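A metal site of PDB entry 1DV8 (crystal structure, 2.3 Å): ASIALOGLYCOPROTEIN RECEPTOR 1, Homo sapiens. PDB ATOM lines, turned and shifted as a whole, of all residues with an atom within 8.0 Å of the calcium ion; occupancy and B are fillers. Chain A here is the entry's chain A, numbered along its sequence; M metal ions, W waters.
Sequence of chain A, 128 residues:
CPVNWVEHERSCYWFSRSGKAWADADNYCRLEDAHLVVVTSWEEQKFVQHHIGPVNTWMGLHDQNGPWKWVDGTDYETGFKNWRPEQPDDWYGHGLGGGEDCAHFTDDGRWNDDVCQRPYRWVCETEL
Along chain A the residues within 4 Å of the calcium ion span positions 38 to 125. The nearest printed residue that does not touch the calcium ion is Tyr 13 (4.2 Å).
The backbone NH of Thr 40 lies close to the side-chain carboxylate of Glu 44 (3.2 Å). The backbone NH of Glu 125 is in hydrogen-bond range of the backbone carbonyl oxygen of His 35 (2.7 Å). The side-chain carboxylate (OE2) of Glu 125 sits close to the side-chain hydroxyl (OG) of Ser 11 (3.2 Å). The side-chain carboxylate (OE1) of Glu 44 sits close to the side-chain hydroxyl (OH) of Tyr 13, at 2.7 Å. The side-chain hydroxyl (OH) of Tyr 13 sits close to the side-chain carboxylate (OE2) of Glu 125 (3.2 Å). OG of Ser 41 lies within hydrogen-bond range of N of Glu 44 (3.3 Å).
The calcium ion is bound by water W2, at 2.1 Å. The calcium ion is bound by the side-chain carboxylate (OE1) of Glu 44, 2.2 Å away. The calcium ion is bound by the backbone carbonyl oxygen (O) of Val 38 (2.2 Å). Water W3 binds the calcium ion (2.5 Å). The calcium ion is bound by water W1 (2.5 Å). The calcium ion is bound by OE2 of Glu 125 (2.5 Å). The calcium ion is bound by the side-chain carboxylate (OE1) of Glu 125, at 2.7 Å. The side-chain carboxylate (OE2) of Glu 44 is bound to the calcium ion.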
ATOM      1  N   HIS A   8     -22.269 -11.940 -18.068  1.00  0.00           N
ATOM      2  CA  HIS A   8     -20.850 -12.087 -18.367  1.00  0.00           C
ATOM      3  C   HIS A   8     -20.082 -10.838 -18.059  1.00  0.00           C
ATOM      4  O   HIS A   8     -20.314  -9.801 -18.671  1.00  0.00           O
ATOM      5  CB  HIS A   8     -20.652 -12.447 -19.833  1.00  0.00           C
ATOM      6  CG  HIS A   8     -19.224 -12.690 -20.196  1.00  0.00           C
ATOM      7  ND1 HIS A   8     -18.512 -13.771 -19.710  1.00  0.00           N
ATOM      8  CD2 HIS A   8     -18.370 -12.000 -20.980  1.00  0.00           C
ATOM      9  CE1 HIS A   8     -17.276 -13.732 -20.191  1.00  0.00           C
ATOM     10  NE2 HIS A   8     -17.166 -12.663 -20.968  1.00  0.00           N
ATOM     11  N   GLU A   9     -19.167 -10.947 -17.103  1.00  0.00           N
ATOM     12  CA  GLU A   9     -18.326  -9.831 -16.691  1.00  0.00           C
ATOM     13  C   GLU A   9     -19.115  -8.561 -16.402  1.00  0.00           C
ATOM     14  O   GLU A   9     -18.803  -7.510 -16.959  1.00  0.00           O
ATOM     15  CB  GLU A   9     -17.273  -9.560 -17.773  1.00  0.00           C
ATOM     16  CG  GLU A   9     -15.853  -9.377 -17.245  1.00  0.00           C
ATOM     17  CD  GLU A   9     -15.281 -10.645 -16.598  1.00  0.00           C
ATOM     18  OE1 GLU A   9     -15.877 -11.132 -15.613  1.00  0.00           O
ATOM     19  OE2 GLU A   9     -14.237 -11.137 -17.072  1.00  0.00           O
ATOM     20  N   SER A  11     -22.209  -7.810 -17.247  1.00  0.00           N
ATOM     21  CA  SER A  11     -23.227  -7.469 -18.234  1.00  0.00           C
ATOM     22  C   SER A  11     -24.211  -8.616 -18.534  1.00  0.00           C
ATOM     23  O   SER A  11     -23.868  -9.795 -18.418  1.00  0.00           O
ATOM     24  CB  SER A  11     -22.582  -7.007 -19.536  1.00  0.00           C
ATOM     25  OG  SER A  11     -21.952  -5.736 -19.399  1.00  0.00           O
ATOM     26  N   CYS A  12     -25.430  -8.253 -18.920  1.00  0.00           N
ATOM     27  CA  CYS A  12     -26.470  -9.209 -19.261  1.00  0.00           C
ATOM     28  C   CYS A  12     -26.730  -9.175 -20.771  1.00  0.00           C
ATOM     29  O   CYS A  12     -26.789  -8.093 -21.376  1.00  0.00           O
ATOM     30  CB  CYS A  12     -27.757  -8.892 -18.509  1.00  0.00           C
ATOM     31  SG  CYS A  12     -27.595  -8.896 -16.697  1.00  0.00           S
ATOM     32  N   TYR A  13     -26.924 -10.356 -21.382  1.00  0.00           N
ATOM     33  CA  TYR A  13     -27.143 -10.437 -22.816  1.00  0.00           C
ATOM     34  C   TYR A  13     -28.300 -11.348 -23.214  1.00  0.00           C
ATOM     35  O   TYR A  13     -28.532 -12.384 -22.599  1.00  0.00           O
ATOM     36  CB  TYR A  13     -25.880 -10.953 -23.528  1.00  0.00           C
ATOM     37  CG  TYR A  13     -24.609 -10.235 -23.176  1.00  0.00           C
ATOM     38  CD1 TYR A  13     -23.993 -10.388 -21.929  1.00  0.00           C
ATOM     39  CD2 TYR A  13     -23.989  -9.396 -24.107  1.00  0.00           C
ATOM     40  CE1 TYR A  13     -22.801  -9.716 -21.616  1.00  0.00           C
ATOM     41  CE2 TYR A  13     -22.809  -8.725 -23.812  1.00  0.00           C
ATOM     42  CZ  TYR A  13     -22.214  -8.887 -22.562  1.00  0.00           C
ATOM     43  OH  TYR A  13     -21.046  -8.203 -22.281  1.00  0.00           O
ATOM     44  N   HIS A  35     -30.104  -2.325 -24.616  1.00  0.00           N
ATOM     45  CA  HIS A  35     -29.625  -1.707 -25.837  1.00  0.00           C
ATOM     46  C   HIS A  35     -28.870  -2.754 -26.643  1.00  0.00           C
ATOM     47  O   HIS A  35     -28.342  -3.704 -26.068  1.00  0.00           O
ATOM     48  CB  HIS A  35     -28.694  -0.545 -25.480  1.00  0.00           C
ATOM     49  CG  HIS A  35     -27.485  -0.967 -24.721  1.00  0.00           C
ATOM     50  ND1 HIS A  35     -26.476  -1.730 -25.282  1.00  0.00           N
ATOM     51  CD2 HIS A  35     -27.110  -0.741 -23.437  1.00  0.00           C
ATOM     52  CE1 HIS A  35     -25.546  -1.955 -24.377  1.00  0.00           C
ATOM     53  NE2 HIS A  35     -25.901  -1.360 -23.251  1.00  0.00           N
ATOM     54  N   LEU A  36     -28.828  -2.582 -27.958  1.00  0.00           N
ATOM     55  CA  LEU A  36     -28.111  -3.524 -28.800  1.00  0.00           C
ATOM     56  C   LEU A  36     -26.700  -3.650 -28.224  1.00  0.00           C
ATOM     57  O   LEU A  36     -26.102  -2.670 -27.765  1.00  0.00           O
ATOM     58  CB  LEU A  36     -28.095  -3.028 -30.258  1.00  0.00           C
ATOM     59  CG  LEU A  36     -29.436  -3.070 -31.003  1.00  0.00           C
ATOM     60  CD1 LEU A  36     -29.320  -2.430 -32.380  1.00  0.00           C
ATOM     61  CD2 LEU A  36     -29.894  -4.522 -31.156  1.00  0.00           C
ATOM     62  N   VAL A  37     -26.174  -4.873 -28.240  1.00  0.00           N
ATOM     63  CA  VAL A  37     -24.864  -5.137 -27.664  1.00  0.00           C
ATOM     64  C   VAL A  37     -23.820  -4.127 -28.100  1.00  0.00           C
ATOM     65  O   VAL A  37     -23.811  -3.686 -29.253  1.00  0.00           O
ATOM     66  CB  VAL A  37     -24.377  -6.587 -28.006  1.00  0.00           C
ATOM     67  CG1 VAL A  37     -24.102  -6.743 -29.504  1.00  0.00           C
ATOM     68  CG2 VAL A  37     -23.154  -6.921 -27.183  1.00  0.00           C
ATOM     69  N   VAL A  38     -22.957  -3.767 -27.154  1.00  0.00           N
ATOM     70  CA  VAL A  38     -21.843  -2.821 -27.335  1.00  0.00           C
ATOM     71  C   VAL A  38     -20.551  -3.563 -26.955  1.00  0.00           C
ATOM     72  O   VAL A  38     -20.313  -3.838 -25.794  1.00  0.00           O
ATOM     73  CB  VAL A  38     -21.992  -1.607 -26.398  1.00  0.00           C
ATOM     74  CG1 VAL A  38     -20.740  -0.742 -26.487  1.00  0.00           C
ATOM     75  CG2 VAL A  38     -23.222  -0.797 -26.793  1.00  0.00           C
ATOM     76  N   VAL A  39     -19.720  -3.874 -27.941  1.00  0.00           N
ATOM     77  CA  VAL A  39     -18.488  -4.614 -27.699  1.00  0.00           C
ATOM     78  C   VAL A  39     -17.259  -3.723 -27.478  1.00  0.00           C
ATOM     79  O   VAL A  39     -16.771  -3.089 -28.414  1.00  0.00           O
ATOM     80  CB  VAL A  39     -18.220  -5.531 -28.881  1.00  0.00           C
ATOM     81  CG1 VAL A  39     -17.112  -6.507 -28.547  1.00  0.00           C
ATOM     82  CG2 VAL A  39     -19.478  -6.273 -29.247  1.00  0.00           C
ATOM     83  N   THR A  40     -16.734  -3.722 -26.253  1.00  0.00           N
ATOM     84  CA  THR A  40     -15.566  -2.893 -25.936  1.00  0.00           C
ATOM     85  C   THR A  40     -14.286  -3.640 -25.543  1.00  0.00           C
ATOM     86  O   THR A  40     -13.392  -3.039 -24.949  1.00  0.00           O
ATOM     87  CB  THR A  40     -15.890  -1.905 -24.820  1.00  0.00           C
ATOM     88  OG1 THR A  40     -16.271  -2.635 -23.641  1.00  0.00           O
ATOM     89  CG2 THR A  40     -17.027  -0.946 -25.241  1.00  0.00           C
ATOM     90  N   SER A  41     -14.185  -4.917 -25.872  1.00  0.00           N
ATOM     91  CA  SER A  41     -12.977  -5.670 -25.560  1.00  0.00           C
ATOM     92  C   SER A  41     -12.949  -7.032 -26.247  1.00  0.00           C
ATOM     93  O   SER A  41     -13.997  -7.618 -26.562  1.00  0.00           O
ATOM     94  CB  SER A  41     -12.832  -5.857 -24.052  1.00  0.00           C
ATOM     95  OG  SER A  41     -13.790  -6.773 -23.561  1.00  0.00           O
ATOM     96  N   GLU A  43     -12.338  -9.934 -25.120  1.00  0.00           N
ATOM     97  CA  GLU A  43     -13.037 -10.966 -24.375  1.00  0.00           C
ATOM     98  C   GLU A  43     -14.544 -10.860 -24.581  1.00  0.00           C
ATOM     99  O   GLU A  43     -15.235 -11.879 -24.643  1.00  0.00           O
ATOM    100  CB  GLU A  43     -12.698 -10.893 -22.882  1.00  0.00           C
ATOM    101  CG  GLU A  43     -13.218  -9.673 -22.139  1.00  0.00           C
ATOM    102  CD  GLU A  43     -14.686  -9.820 -21.716  1.00  0.00           C
ATOM    103  OE1 GLU A  43     -15.268  -8.847 -21.175  1.00  0.00           O
ATOM    104  OE2 GLU A  43     -15.240 -10.920 -21.933  1.00  0.00           O
ATOM    105  N   GLU A  44     -15.077  -9.631 -24.695  1.00  0.00           N
ATOM    106  CA  GLU A  44     -16.510  -9.471 -24.902  1.00  0.00           C
ATOM    107  C   GLU A  44     -16.872  -9.923 -26.326  1.00  0.00           C
ATOM    108  O   GLU A  44     -17.918 -10.520 -26.555  1.00  0.00           O
ATOM    109  CB  GLU A  44     -16.954  -8.020 -24.675  1.00  0.00           C
ATOM    110  CG  GLU A  44     -18.488  -7.872 -24.664  1.00  0.00           C
ATOM    111  CD  GLU A  44     -18.996  -6.505 -24.247  1.00  0.00           C
ATOM    112  OE1 GLU A  44     -20.231  -6.381 -24.038  1.00  0.00           O
ATOM    113  OE2 GLU A  44     -18.185  -5.561 -24.130  1.00  0.00           O
ATOM    114  N   GLN A  45     -15.981  -9.630 -27.258  1.00  0.00           N
ATOM    115  CA  GLN A  45     -16.182 -10.043 -28.640  1.00  0.00           C
ATOM    116  C   GLN A  45     -16.189 -11.580 -28.667  1.00  0.00           C
ATOM    117  O   GLN A  45     -17.124 -12.194 -29.174  1.00  0.00           O
ATOM    118  CB  GLN A  45     -15.043  -9.492 -29.525  1.00  0.00           C
ATOM    119  CG  GLN A  45     -14.869 -10.152 -30.912  1.00  0.00           C
ATOM    120  CD  GLN A  45     -15.907  -9.732 -31.962  1.00  0.00           C
ATOM    121  OE1 GLN A  45     -16.266  -8.551 -32.083  1.00  0.00           O
ATOM    122  NE2 GLN A  45     -16.384 -10.705 -32.737  1.00  0.00           N
ATOM    123  N   VAL A  48     -19.333 -13.047 -27.528  1.00  0.00           N
ATOM    124  CA  VAL A  48     -20.496 -12.979 -28.409  1.00  0.00           C
ATOM    125  C   VAL A  48     -20.428 -13.916 -29.602  1.00  0.00           C
ATOM    126  O   VAL A  48     -21.449 -14.505 -29.982  1.00  0.00           O
ATOM    127  CB  VAL A  48     -20.710 -11.551 -28.893  1.00  0.00           C
ATOM    128  CG1 VAL A  48     -21.842 -11.507 -29.940  1.00  0.00           C
ATOM    129  CG2 VAL A  48     -21.046 -10.682 -27.709  1.00  0.00           C
ATOM    130  N   TRP A  70     -21.970   3.993 -30.707  1.00  0.00           N
ATOM    131  CA  TRP A  70     -22.493   2.825 -30.051  1.00  0.00           C
ATOM    132  C   TRP A  70     -23.732   3.380 -29.399  1.00  0.00           C
ATOM    133  O   TRP A  70     -23.680   4.465 -28.836  1.00  0.00           O
ATOM    134  CB  TRP A  70     -21.506   2.316 -29.009  1.00  0.00           C
ATOM    135  CG  TRP A  70     -20.315   1.634 -29.595  1.00  0.00           C
ATOM    136  CD1 TRP A  70     -19.061   2.163 -29.740  1.00  0.00           C
ATOM    137  CD2 TRP A  70     -20.242   0.288 -30.055  1.00  0.00           C
ATOM    138  NE1 TRP A  70     -18.209   1.214 -30.257  1.00  0.00           N
ATOM    139  CE2 TRP A  70     -18.908   0.054 -30.463  1.00  0.00           C
ATOM    140  CE3 TRP A  70     -21.177  -0.746 -30.180  1.00  0.00           C
ATOM    141  CZ2 TRP A  70     -18.479  -1.192 -30.952  1.00  0.00           C
ATOM    142  CZ3 TRP A  70     -20.753  -1.986 -30.687  1.00  0.00           C
ATOM    143  CH2 TRP A  70     -19.410  -2.190 -31.075  1.00  0.00           C
ATOM    144  N   ASP A  72     -25.118   3.233 -26.779  1.00  0.00           N
ATOM    145  CA  ASP A  72     -25.110   3.601 -25.365  1.00  0.00           C
ATOM    146  C   ASP A  72     -24.219   4.811 -25.110  1.00  0.00           C
ATOM    147  O   ASP A  72     -24.033   5.224 -23.972  1.00  0.00           O
ATOM    148  CB  ASP A  72     -24.627   2.432 -24.514  1.00  0.00           C
ATOM    149  CG  ASP A  72     -23.142   2.232 -24.621  1.00  0.00           C
ATOM    150  OD1 ASP A  72     -22.578   2.670 -25.637  1.00  0.00           O
ATOM    151  OD2 ASP A  72     -22.550   1.622 -23.717  1.00  0.00           O
ATOM    152  N   THR A  74     -20.942   4.908 -25.739  1.00  0.00           N
ATOM    153  CA  THR A  74     -19.531   4.557 -25.589  1.00  0.00           C
ATOM    154  C   THR A  74     -18.781   5.142 -26.775  1.00  0.00           C
ATOM    155  O   THR A  74     -19.291   5.131 -27.897  1.00  0.00           O
ATOM    156  CB  THR A  74     -19.349   3.030 -25.539  1.00  0.00           C
ATOM    157  OG1 THR A  74     -19.959   2.520 -24.345  1.00  0.00           O
ATOM    158  CG2 THR A  74     -17.859   2.667 -25.565  1.00  0.00           C
ATOM    159  N   GLU A 125     -28.129  -6.056 -24.671  1.00  0.00           N
ATOM    160  CA  GLU A 125     -27.208  -6.025 -23.550  1.00  0.00           C
ATOM    161  C   GLU A 125     -27.627  -4.982 -22.516  1.00  0.00           C
ATOM    162  O   GLU A 125     -28.234  -3.959 -22.857  1.00  0.00           O
ATOM    163  CB  GLU A 125     -25.782  -5.698 -24.022  1.00  0.00           C
ATOM    164  CG  GLU A 125     -24.873  -5.196 -22.899  1.00  0.00           C
ATOM    165  CD  GLU A 125     -23.408  -4.979 -23.304  1.00  0.00           C
ATOM    166  OE1 GLU A 125     -23.157  -4.413 -24.382  1.00  0.00           O
ATOM    167  OE2 GLU A 125     -22.494  -5.367 -22.527  1.00  0.00           O
ATOM    168  N   THR A 126     -27.330  -5.267 -21.253  1.00  0.00           N
ATOM    169  CA  THR A 126     -27.617  -4.351 -20.166  1.00  0.00           C
ATOM    170  C   THR A 126     -26.537  -4.565 -19.115  1.00  0.00           C
ATOM    171  O   THR A 126     -26.145  -5.696 -18.850  1.00  0.00           O
ATOM    172  CB  THR A 126     -28.995  -4.599 -19.566  1.00  0.00           C
ATOM    173  OG1 THR A 126     -29.358  -3.460 -18.770  1.00  0.00           O
ATOM    174  CG2 THR A 126     -29.014  -5.840 -18.719  1.00  0.00           C
ATOM    175  N   GLU A 127     -26.032  -3.473 -18.537  1.00  0.00           N
ATOM    176  CA  GLU A 127     -24.976  -3.593 -17.530  1.00  0.00           C
ATOM    177  C   GLU A 127     -25.490  -3.633 -16.101  1.00  0.00           C
ATOM    178  O   GLU A 127     -26.561  -3.098 -15.791  1.00  0.00           O
ATOM    179  CB  GLU A 127     -23.971  -2.435 -17.636  1.00  0.00           C
ATOM    180  CG  GLU A 127     -23.226  -2.347 -18.952  1.00  0.00           C
ATOM    181  CD  GLU A 127     -24.033  -1.660 -20.015  1.00  0.00           C
ATOM    182  OE1 GLU A 127     -23.629  -1.670 -21.192  1.00  0.00           O
ATOM    183  OE2 GLU A 127     -25.089  -1.102 -19.667  1.00  0.00           O
HETATM  184 CA    CA M   1     -20.559  -4.278 -23.666  1.00  0.00          CA
HETATM  185  O   HOH W   1     -19.338  -4.681 -21.555  1.00  0.00           O
HETATM  186  O   HOH W   2     -21.712  -2.886 -22.572  1.00  0.00           O
HETATM  187  O   HOH W   3     -18.997  -2.436 -23.240  1.00  0.00           O
